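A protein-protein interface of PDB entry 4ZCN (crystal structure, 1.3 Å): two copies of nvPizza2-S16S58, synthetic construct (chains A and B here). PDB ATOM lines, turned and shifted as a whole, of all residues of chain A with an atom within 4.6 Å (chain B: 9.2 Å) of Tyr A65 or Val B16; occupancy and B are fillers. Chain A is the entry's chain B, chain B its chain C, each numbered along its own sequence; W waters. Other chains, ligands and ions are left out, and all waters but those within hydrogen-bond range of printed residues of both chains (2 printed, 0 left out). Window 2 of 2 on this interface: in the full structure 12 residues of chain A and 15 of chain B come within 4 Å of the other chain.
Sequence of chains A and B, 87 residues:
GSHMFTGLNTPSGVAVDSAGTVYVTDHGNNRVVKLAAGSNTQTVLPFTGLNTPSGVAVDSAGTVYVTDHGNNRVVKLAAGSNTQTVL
OXT of Leu A87 sits at hydrogen-bond distance from N of Phe B5, 3.2 Å away.
Hydrophobic or aromatic side chains of chain B within 4 Å of the printed part of chain A: Phe B5, Val B14, Val B16, Val B22 and Leu B35.
Hydrophobic or aromatic side chains of chain A that line the printed part of chain B: Ala A57, Tyr A65 and Leu A87.
Among the printed residues, no Asp or Glu carboxylate lies within 4 Å of a Lys or Arg side-chain nitrogen of the other chain.
Tyr A65 touches just these residues of chain B: Val B14, Val B16 and Val B22.
Val B16 touches just one residue of chain A: Tyr A65.
Ala A57 touches just one residue of chain B: Val B14.
No residue of chain B comes within 4 Å of Val A66.
Of the printed residues of chain A, Val B14 touches Val A56 (3.9 Å), Ala A57 (3.5 Å), Tyr A65 (3.7 Å) and Thr A67 (3.8 Å).
Of the printed residues of chain A, Phe B5 touches Leu A87.
Of the printed residues of chain A, Leu B35 touches Leu A87.
Of the printed residues of chain A, Gly B13 touches Thr A67 (3.4 Å).
Lys A76 touches none of the printed residues of chain B.
Ser B18 touches none of the printed residues of chain A.
The nearest residue of chain B that does not touch Tyr A65 is Gly B20 (5.0 Å).
The nearest residue of chain A that does not touch Val B16 is Asp A59 (4.1 Å).
The nearest printed residue of chain A that does not touch Val B14 is Gly A55 (4.1 Å).
5 positions are printed for both chains.
Of the 10 pairs that touch across the chains among the printed residues, none has its exchanged pair printed and touching as well.
Water W1 bridges O of Val B14 (2.8 Å) and O of Val A56 (3.5 Å).
Water W2 bridges the side-chain hydroxyl (OH) of Tyr A65 (2.8 Å) and the backbone carbonyl oxygen (O) of Gly B20 (2.8 Å).
The backbone NH (N) of Leu B35 is in hydrogen-bond range of the backbone carbonyl oxygen (O) of Val B22, 2.9 Å away.
The backbone NH (N) of Gly A55 lies within hydrogen-bond range of the side-chain hydroxyl (OG1) of Thr A67 (3.0 Å).
OD2 of Asp A59 sits at hydrogen-bond distance from OH of Tyr A65 (2.8 Å).
The backbone carbonyl oxygen (O) of Ala A57 sits at hydrogen-bond distance from the backbone NH (N) of Tyr A65 (2.8 Å).
Among the printed residues, merely in contact across the chains: Val A56 with Val B14 (3.9 Å), Ala A57 with Val B14 (3.5 Å), Tyr A65 with Val B14 (3.7 Å), Tyr A65 with Val B16 (3.6 Å), Tyr A65 with Val B22 (3.6 Å), Thr A67 with Gly B13 (3.4 Å), Thr A67 with Val B14 (3.8 Å), Leu A87 with Val B22 (3.8 Å) and Leu A87 with Leu B35 (3.7 Å).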
ATOM      1  N   GLY A  55      18.837  -8.278   1.200  1.00  0.00           N
ATOM      2  CA  GLY A  55      17.424  -8.594   1.103  1.00  0.00           C
ATOM      3  C   GLY A  55      16.796  -8.832   2.456  1.00  0.00           C
ATOM      4  O   GLY A  55      17.496  -9.077   3.442  1.00  0.00           O
ATOM      5  N   VAL A  56      15.469  -8.794   2.492  1.00  0.00           N
ATOM      6  CA  VAL A  56      14.744  -8.887   3.748  1.00  0.00           C
ATOM      7  C   VAL A  56      13.403  -9.563   3.528  1.00  0.00           C
ATOM      8  O   VAL A  56      12.800  -9.431   2.457  1.00  0.00           O
ATOM      9  CB  VAL A  56      14.555  -7.469   4.388  1.00  0.00           C
ATOM     10  CG1 VAL A  56      13.912  -6.487   3.391  1.00  0.00           C
ATOM     11  CG2 VAL A  56      13.771  -7.528   5.687  1.00  0.00           C
ATOM     12  N   ALA A  57      12.958 -10.314   4.529  1.00  0.00           N
ATOM     13  CA  ALA A  57      11.622 -10.900   4.548  1.00  0.00           C
ATOM     14  C   ALA A  57      11.067 -10.772   5.954  1.00  0.00           C
ATOM     15  O   ALA A  57      11.832 -10.657   6.919  1.00  0.00           O
ATOM     16  CB  ALA A  57      11.652 -12.357   4.123  1.00  0.00           C
ATOM     17  N   ASP A  59       8.013 -12.613   8.468  1.00  0.00           N
ATOM     18  CA  ASP A  59       6.972 -13.637   8.566  1.00  0.00           C
ATOM     19  C   ASP A  59       5.747 -13.116   9.329  1.00  0.00           C
ATOM     20  O   ASP A  59       5.704 -11.954   9.741  1.00  0.00           O
ATOM     21  CB  ASP A  59       7.516 -14.940   9.193  1.00  0.00           C
ATOM     22  CG  ASP A  59       7.896 -14.813  10.669  1.00  0.00           C
ATOM     23  OD1 ASP A  59       7.497 -13.848  11.351  1.00  0.00           O
ATOM     24  OD2 ASP A  59       8.590 -15.733  11.162  1.00  0.00           O
ATOM     25  N   THR A  63       8.775 -11.512  12.635  1.00  0.00           N
ATOM     26  CA  THR A  63      10.201 -11.791  12.681  1.00  0.00           C
ATOM     27  C   THR A  63      10.833 -11.380  11.363  1.00  0.00           C
ATOM     28  O   THR A  63      10.284 -11.658  10.298  1.00  0.00           O
ATOM     29  CB  THR A  63      10.468 -13.265  12.972  1.00  0.00           C
ATOM     30  OG1 THR A  63       9.952 -13.570  14.273  1.00  0.00           O
ATOM     31  CG2 THR A  63      11.963 -13.568  12.932  1.00  0.00           C
ATOM     32  N   VAL A  64      11.966 -10.685  11.451  1.00  0.00           N
ATOM     33  CA  VAL A  64      12.618 -10.072  10.299  1.00  0.00           C
ATOM     34  C   VAL A  64      13.843 -10.877   9.901  1.00  0.00           C
ATOM     35  O   VAL A  64      14.720 -11.105  10.720  1.00  0.00           O
ATOM     36  CB  VAL A  64      13.027  -8.610  10.597  1.00  0.00           C
ATOM     37  CG1 VAL A  64      13.690  -7.977   9.378  1.00  0.00           C
ATOM     38  CG2 VAL A  64      11.815  -7.795  11.047  1.00  0.00           C
ATOM     39  N   TYR A  65      13.874 -11.328   8.654  1.00  0.00           N
ATOM     40  CA  TYR A  65      14.957 -12.157   8.133  1.00  0.00           C
ATOM     41  C   TYR A  65      15.762 -11.351   7.140  1.00  0.00           C
ATOM     42  O   TYR A  65      15.186 -10.685   6.282  1.00  0.00           O
ATOM     43  CB  TYR A  65      14.421 -13.411   7.441  1.00  0.00           C
ATOM     44  CG  TYR A  65      13.554 -14.313   8.290  1.00  0.00           C
ATOM     45  CD1 TYR A  65      12.261 -13.938   8.630  1.00  0.00           C
ATOM     46  CD2 TYR A  65      14.009 -15.561   8.708  1.00  0.00           C
ATOM     47  CE1 TYR A  65      11.456 -14.761   9.389  1.00  0.00           C
ATOM     48  CE2 TYR A  65      13.207 -16.394   9.460  1.00  0.00           C
ATOM     49  CZ  TYR A  65      11.931 -15.988   9.796  1.00  0.00           C
ATOM     50  OH  TYR A  65      11.128 -16.815  10.546  1.00  0.00           O
ATOM     51  N   VAL A  66      17.085 -11.428   7.225  1.00  0.00           N
ATOM     52  CA  VAL A  66      17.935 -10.620   6.372  1.00  0.00           C
ATOM     53  C   VAL A  66      19.062 -11.461   5.782  1.00  0.00           C
ATOM     54  O   VAL A  66      19.694 -12.240   6.502  1.00  0.00           O
ATOM     55  CB  VAL A  66      18.510  -9.420   7.164  1.00  0.00           C
ATOM     56  CG1 VAL A  66      19.568  -8.688   6.366  1.00  0.00           C
ATOM     57  CG2 VAL A  66      17.383  -8.471   7.555  1.00  0.00           C
ATOM     58  N   THR A  67      19.294 -11.326   4.477  1.00  0.00           N
ATOM     59  CA  THR A  67      20.491 -11.891   3.881  1.00  0.00           C
ATOM     60  C   THR A  67      21.637 -10.914   4.108  1.00  0.00           C
ATOM     61  O   THR A  67      21.685  -9.816   3.543  1.00  0.00           O
ATOM     62  CB  THR A  67      20.311 -12.210   2.389  1.00  0.00           C
ATOM     63  OG1 THR A  67      19.529 -11.194   1.754  1.00  0.00           O
ATOM     64  CG2 THR A  67      19.601 -13.544   2.221  1.00  0.00           C
ATOM     65  N   VAL A  75      20.394 -13.864   8.809  1.00  0.00           N
ATOM     66  CA  VAL A  75      20.108 -13.635  10.219  1.00  0.00           C
ATOM     67  C   VAL A  75      18.642 -13.290  10.404  1.00  0.00           C
ATOM     68  O   VAL A  75      17.982 -12.846   9.460  1.00  0.00           O
ATOM     69  CB  VAL A  75      20.990 -12.509  10.808  1.00  0.00           C
ATOM     70  CG1 VAL A  75      22.468 -12.898  10.761  1.00  0.00           C
ATOM     71  CG2 VAL A  75      20.764 -11.206  10.073  1.00  0.00           C
ATOM     72  N   LYS A  76      18.117 -13.516  11.605  1.00  0.00           N
ATOM     73  CA  LYS A  76      16.757 -13.092  11.895  1.00  0.00           C
ATOM     74  C   LYS A  76      16.661 -12.420  13.254  1.00  0.00           C
ATOM     75  O   LYS A  76      17.490 -12.619  14.146  1.00  0.00           O
ATOM     76  CB  LYS A  76      15.784 -14.267  11.825  1.00  0.00           C
ATOM     77  CG  LYS A  76      15.905 -15.222  12.977  1.00  0.00           C
ATOM     78  CD  LYS A  76      14.918 -16.367  12.856  1.00  0.00           C
ATOM     79  CE  LYS A  76      15.105 -17.379  13.966  1.00  0.00           C
ATOM     80  NZ  LYS A  76      14.104 -18.474  13.836  1.00  0.00           N
ATOM     81  N   LEU A  87      20.964 -17.959  11.084  1.00  0.00           N
ATOM     82  CA  LEU A  87      20.294 -19.164  10.580  1.00  0.00           C
ATOM     83  C   LEU A  87      21.261 -20.200  10.028  1.00  0.00           C
ATOM     84  O   LEU A  87      22.288 -19.856   9.444  1.00  0.00           O
ATOM     85  CB  LEU A  87      19.279 -18.806   9.494  1.00  0.00           C
ATOM     86  CG  LEU A  87      17.919 -18.255   9.927  1.00  0.00           C
ATOM     87  CD1 LEU A  87      18.041 -16.837  10.446  1.00  0.00           C
ATOM     88  CD2 LEU A  87      16.962 -18.310   8.762  1.00  0.00           C
ATOM     89  OXT LEU A  87      21.011 -21.404  10.141  1.00  0.00           O
ATOM     90  N   PHE B   5      22.611 -22.916   7.831  1.00  0.00           N
ATOM     91  CA  PHE B   5      22.902 -22.699   6.407  1.00  0.00           C
ATOM     92  C   PHE B   5      24.404 -22.889   6.261  1.00  0.00           C
ATOM     93  O   PHE B   5      25.171 -22.536   7.160  1.00  0.00           O
ATOM     94  CB  PHE B   5      22.491 -21.309   5.894  1.00  0.00           C
ATOM     95  CG  PHE B   5      21.036 -21.191   5.497  1.00  0.00           C
ATOM     96  CD1 PHE B   5      20.495 -21.994   4.500  1.00  0.00           C
ATOM     97  CD2 PHE B   5      20.217 -20.249   6.101  1.00  0.00           C
ATOM     98  CE1 PHE B   5      19.157 -21.870   4.132  1.00  0.00           C
ATOM     99  CE2 PHE B   5      18.880 -20.118   5.735  1.00  0.00           C
ATOM    100  CZ  PHE B   5      18.349 -20.923   4.754  1.00  0.00           C
ATOM    101  N   GLY B  13      18.901 -12.796  -1.611  1.00  0.00           N
ATOM    102  CA  GLY B  13      17.509 -12.621  -1.227  1.00  0.00           C
ATOM    103  C   GLY B  13      17.014 -13.715  -0.306  1.00  0.00           C
ATOM    104  O   GLY B  13      17.601 -14.802  -0.238  1.00  0.00           O
ATOM    105  N   VAL B  14      15.932 -13.427   0.405  1.00  0.00           N
ATOM    106  CA  VAL B  14      15.343 -14.386   1.329  1.00  0.00           C
ATOM    107  C   VAL B  14      13.811 -14.286   1.304  1.00  0.00           C
ATOM    108  O   VAL B  14      13.261 -13.205   1.129  1.00  0.00           O
ATOM    109  CB  VAL B  14      15.881 -14.153   2.775  1.00  0.00           C
ATOM    110  CG1 VAL B  14      15.656 -12.693   3.238  1.00  0.00           C
ATOM    111  CG2 VAL B  14      15.287 -15.151   3.759  1.00  0.00           C
ATOM    112  N   ALA B  15      13.133 -15.424   1.447  1.00  0.00           N
ATOM    113  CA  ALA B  15      11.676 -15.466   1.545  1.00  0.00           C
ATOM    114  C   ALA B  15      11.309 -16.492   2.606  1.00  0.00           C
ATOM    115  O   ALA B  15      12.079 -17.412   2.856  1.00  0.00           O
ATOM    116  CB  ALA B  15      11.051 -15.831   0.213  1.00  0.00           C
ATOM    117  N   VAL B  16      10.148 -16.338   3.237  1.00  0.00           N
ATOM    118  CA  VAL B  16       9.727 -17.271   4.278  1.00  0.00           C
ATOM    119  C   VAL B  16       8.289 -17.680   3.995  1.00  0.00           C
ATOM    120  O   VAL B  16       7.444 -16.811   3.761  1.00  0.00           O
ATOM    121  CB  VAL B  16       9.854 -16.643   5.692  1.00  0.00           C
ATOM    122  CG1 VAL B  16       9.475 -17.649   6.777  1.00  0.00           C
ATOM    123  CG2 VAL B  16      11.263 -16.150   5.922  1.00  0.00           C
ATOM    124  N   ASP B  17       8.002 -18.983   3.980  1.00  0.00           N
ATOM    125  CA  ASP B  17       6.640 -19.401   3.647  1.00  0.00           C
ATOM    126  C   ASP B  17       5.795 -19.594   4.900  1.00  0.00           C
ATOM    127  O   ASP B  17       6.260 -19.369   6.020  1.00  0.00           O
ATOM    128  CB  ASP B  17       6.633 -20.666   2.769  1.00  0.00           C
ATOM    129  CG  ASP B  17       7.100 -21.931   3.497  1.00  0.00           C
ATOM    130  OD1 ASP B  17       7.182 -21.974   4.742  1.00  0.00           O
ATOM    131  OD2 ASP B  17       7.385 -22.915   2.785  1.00  0.00           O
ATOM    132  N   SER B  18       4.544 -19.990   4.699  1.00  0.00           N
ATOM    133  CA  SER B  18       3.595 -20.089   5.802  1.00  0.00           C
ATOM    134  C   SER B  18       3.996 -21.137   6.843  1.00  0.00           C
ATOM    135  O   SER B  18       3.577 -21.062   7.995  1.00  0.00           O
ATOM    136  CB  SER B  18       2.194 -20.397   5.267  1.00  0.00           C
ATOM    137  OG  SER B  18       2.120 -21.719   4.765  1.00  0.00           O
ATOM    138  N   ALA B  19       4.808 -22.106   6.440  1.00  0.00           N
ATOM    139  CA  ALA B  19       5.282 -23.131   7.364  1.00  0.00           C
ATOM    140  C   ALA B  19       6.562 -22.711   8.087  1.00  0.00           C
ATOM    141  O   ALA B  19       7.111 -23.480   8.869  1.00  0.00           O
ATOM    142  CB  ALA B  19       5.508 -24.453   6.620  1.00  0.00           C
ATOM    143  N   GLY B  20       7.046 -21.500   7.823  1.00  0.00           N
ATOM    144  CA  GLY B  20       8.265 -21.022   8.451  1.00  0.00           C
ATOM    145  C   GLY B  20       9.537 -21.484   7.763  1.00  0.00           C
ATOM    146  O   GLY B  20      10.633 -21.300   8.283  1.00  0.00           O
ATOM    147  N   THR B  21       9.398 -22.097   6.593  1.00  0.00           N
ATOM    148  CA  THR B  21      10.568 -22.503   5.827  1.00  0.00           C
ATOM    149  C   THR B  21      11.214 -21.272   5.208  1.00  0.00           C
ATOM    150  O   THR B  21      10.521 -20.423   4.637  1.00  0.00           O
ATOM    151  CB  THR B  21      10.204 -23.520   4.732  1.00  0.00           C
ATOM    152  OG1 THR B  21       9.683 -24.706   5.344  1.00  0.00           O
ATOM    153  CG2 THR B  21      11.420 -23.886   3.891  1.00  0.00           C
ATOM    154  N   VAL B  22      12.540 -21.186   5.309  1.00  0.00           N
ATOM    155  CA  VAL B  22      13.290 -20.044   4.813  1.00  0.00           C
ATOM    156  C   VAL B  22      13.997 -20.412   3.516  1.00  0.00           C
ATOM    157  O   VAL B  22      14.671 -21.434   3.454  1.00  0.00           O
ATOM    158  CB  VAL B  22      14.320 -19.567   5.860  1.00  0.00           C
ATOM    159  CG1 VAL B  22      15.122 -18.397   5.326  1.00  0.00           C
ATOM    160  CG2 VAL B  22      13.619 -19.190   7.183  1.00  0.00           C
ATOM    161  N   TYR B  23      13.822 -19.577   2.493  1.00  0.00           N
ATOM    162  CA  TYR B  23      14.404 -19.772   1.172  1.00  0.00           C
ATOM    163  C   TYR B  23      15.425 -18.692   0.903  1.00  0.00           C
ATOM    164  O   TYR B  23      15.165 -17.526   1.176  1.00  0.00           O
ATOM    165  CB  TYR B  23      13.334 -19.723   0.078  1.00  0.00           C
ATOM    166  CG  TYR B  23      12.247 -20.759   0.241  1.00  0.00           C
ATOM    167  CD1 TYR B  23      11.165 -20.520   1.073  1.00  0.00           C
ATOM    168  CD2 TYR B  23      12.299 -21.970  -0.441  1.00  0.00           C
ATOM    169  CE1 TYR B  23      10.170 -21.456   1.234  1.00  0.00           C
ATOM    170  CE2 TYR B  23      11.308 -22.911  -0.285  1.00  0.00           C
ATOM    171  CZ  TYR B  23      10.243 -22.647   0.551  1.00  0.00           C
ATOM    172  OH  TYR B  23       9.252 -23.584   0.710  1.00  0.00           O
ATOM    173  N   VAL B  24      16.586 -19.068   0.382  1.00  0.00           N
ATOM    174  CA  VAL B  24      17.645 -18.108   0.119  1.00  0.00           C
ATOM    175  C   VAL B  24      18.225 -18.305  -1.265  1.00  0.00           C
ATOM    176  O   VAL B  24      18.560 -19.438  -1.656  1.00  0.00           O
ATOM    177  CB  VAL B  24      18.773 -18.228   1.152  1.00  0.00           C
ATOM    178  CG1 VAL B  24      19.914 -17.280   0.817  1.00  0.00           C
ATOM    179  CG2 VAL B  24      18.235 -17.983   2.552  1.00  0.00           C
ATOM    180  N   LYS B  34      16.922 -24.060   0.908  1.00  0.00           N
ATOM    181  CA  LYS B  34      15.902 -23.841   1.910  1.00  0.00           C
ATOM    182  C   LYS B  34      16.269 -24.529   3.213  1.00  0.00           C
ATOM    183  O   LYS B  34      17.067 -25.476   3.248  1.00  0.00           O
ATOM    184  CB  LYS B  34      14.540 -24.326   1.428  1.00  0.00           C
ATOM    185  CG  LYS B  34      14.408 -25.838   1.400  1.00  0.00           C
ATOM    186  CD  LYS B  34      12.981 -26.242   1.088  1.00  0.00           C
ATOM    187  CE  LYS B  34      12.840 -27.746   1.041  1.00  0.00           C
ATOM    188  NZ  LYS B  34      11.429 -28.133   0.794  1.00  0.00           N
ATOM    189  N   LEU B  35      15.679 -24.024   4.286  1.00  0.00           N
ATOM    190  CA  LEU B  35      15.860 -24.589   5.605  1.00  0.00           C
ATOM    191  C   LEU B  35      14.500 -24.591   6.272  1.00  0.00           C
ATOM    192  O   LEU B  35      13.943 -23.525   6.555  1.00  0.00           O
ATOM    193  CB  LEU B  35      16.872 -23.775   6.405  1.00  0.00           C
ATOM    194  CG  LEU B  35      17.405 -24.330   7.718  1.00  0.00           C
ATOM    195  CD1 LEU B  35      18.162 -25.633   7.485  1.00  0.00           C
ATOM    196  CD2 LEU B  35      18.293 -23.283   8.379  1.00  0.00           C
ATOM    197  N   ALA B  36      13.959 -25.783   6.508  1.00  0.00           N
ATOM    198  CA  ALA B  36      12.664 -25.905   7.161  1.00  0.00           C
ATOM    199  C   ALA B  36      12.823 -25.575   8.637  1.00  0.00           C
ATOM    200  O   ALA B  36      13.922 -25.700   9.190  1.00  0.00           O
ATOM    201  CB  ALA B  36      12.095 -27.305   6.979  1.00  0.00           C
ATOM    202  N   ALA B  37      11.735 -25.139   9.266  1.00  0.00           N
ATOM    203  CA  ALA B  37      11.738 -24.897  10.701  1.00  0.00           C
ATOM    204  C   ALA B  37      12.223 -26.152  11.418  1.00  0.00           C
ATOM    205  O   ALA B  37      11.767 -27.259  11.128  1.00  0.00           O
ATOM    206  CB  ALA B  37      10.350 -24.499  11.187  1.00  0.00           C
ATOM    207  N   VAL B  56      14.140 -13.787  -4.551  1.00  0.00           N
ATOM    208  CA  VAL B  56      13.242 -14.914  -4.384  1.00  0.00           C
ATOM    209  C   VAL B  56      11.957 -14.445  -3.708  1.00  0.00           C
ATOM    210  O   VAL B  56      11.975 -13.505  -2.918  1.00  0.00           O
ATOM    211  CB  VAL B  56      13.932 -16.041  -3.553  1.00  0.00           C
ATOM    212  CG1 VAL B  56      14.401 -15.521  -2.190  1.00  0.00           C
ATOM    213  CG2 VAL B  56      13.025 -17.278  -3.395  1.00  0.00           C
ATOM    214  N   ALA B  57      10.843 -15.077  -4.057  1.00  0.00           N
ATOM    215  CA  ALA B  57       9.578 -14.851  -3.384  1.00  0.00           C
ATOM    216  C   ALA B  57       8.867 -16.185  -3.259  1.00  0.00           C
ATOM    217  O   ALA B  57       9.095 -17.098  -4.059  1.00  0.00           O
ATOM    218  CB  ALA B  57       8.720 -13.855  -4.152  1.00  0.00           C
ATOM    219  N   VAL B  58       8.003 -16.303  -2.263  1.00  0.00           N
ATOM    220  CA  VAL B  58       7.170 -17.490  -2.152  1.00  0.00           C
ATOM    221  C   VAL B  58       5.744 -17.039  -1.897  1.00  0.00           C
ATOM    222  O   VAL B  58       5.510 -16.092  -1.133  1.00  0.00           O
ATOM    223  CB  VAL B  58       7.659 -18.454  -1.041  1.00  0.00           C
ATOM    224  CG1 VAL B  58       7.628 -17.784   0.337  1.00  0.00           C
ATOM    225  CG2 VAL B  58       6.840 -19.740  -1.036  1.00  0.00           C
ATOM    226  N   ASP B  59       4.789 -17.667  -2.570  1.00  0.00           N
ATOM    227  CA  ASP B  59       3.407 -17.252  -2.371  1.00  0.00           C
ATOM    228  C   ASP B  59       2.687 -18.194  -1.404  1.00  0.00           C
ATOM    229  O   ASP B  59       3.280 -19.130  -0.860  1.00  0.00           O
ATOM    230  CB  ASP B  59       2.657 -17.113  -3.715  1.00  0.00           C
ATOM    231  CG  ASP B  59       2.438 -18.431  -4.464  1.00  0.00           C
ATOM    232  OD1 ASP B  59       2.574 -19.535  -3.901  1.00  0.00           O
ATOM    233  OD2 ASP B  59       2.072 -18.334  -5.656  1.00  0.00           O
ATOM    234  N   SER B  60       1.412 -17.910  -1.165  1.00  0.00           N
ATOM    235  CA  SER B  60       0.639 -18.630  -0.163  1.00  0.00           C
ATOM    236  C   SER B  60       0.246 -20.037  -0.621  1.00  0.00           C
ATOM    237  O   SER B  60      -0.308 -20.811   0.156  1.00  0.00           O
ATOM    238  CB  SER B  60      -0.613 -17.831   0.210  1.00  0.00           C
ATOM    239  OG  SER B  60      -1.384 -17.540  -0.938  1.00  0.00           O
ATOM    240  N   GLY B  62       2.712 -21.865  -1.866  1.00  0.00           N
ATOM    241  CA  GLY B  62       3.997 -22.525  -1.715  1.00  0.00           C
ATOM    242  C   GLY B  62       4.897 -22.489  -2.937  1.00  0.00           C
ATOM    243  O   GLY B  62       5.955 -23.117  -2.950  1.00  0.00           O
ATOM    244  N   THR B  63       4.478 -21.758  -3.966  1.00  0.00           N
ATOM    245  CA  THR B  63       5.280 -21.633  -5.177  1.00  0.00           C
ATOM    246  C   THR B  63       6.432 -20.674  -4.939  1.00  0.00           C
ATOM    247  O   THR B  63       6.238 -19.589  -4.391  1.00  0.00           O
ATOM    248  CB  THR B  63       4.432 -21.140  -6.368  1.00  0.00           C
ATOM    249  OG1 THR B  63       3.384 -22.080  -6.627  1.00  0.00           O
ATOM    250  CG2 THR B  63       5.279 -20.980  -7.621  1.00  0.00           C
ATOM    251  N   VAL B  64       7.624 -21.096  -5.344  1.00  0.00           N
ATOM    252  CA  VAL B  64       8.849 -20.328  -5.175  1.00  0.00           C
ATOM    253  C   VAL B  64       9.241 -19.702  -6.503  1.00  0.00           C
ATOM    254  O   VAL B  64       9.343 -20.389  -7.511  1.00  0.00           O
ATOM    255  CB  VAL B  64      10.013 -21.217  -4.635  1.00  0.00           C
ATOM    256  CG1 VAL B  64      11.305 -20.398  -4.499  1.00  0.00           C
ATOM    257  CG2 VAL B  64       9.633 -21.849  -3.294  1.00  0.00           C
HETATM  258  O   HOH W   1      14.386 -11.044  -0.155  1.00  0.00           O
HETATM  259  O   HOH W   2      11.324 -19.630  10.483  1.00  0.00           O
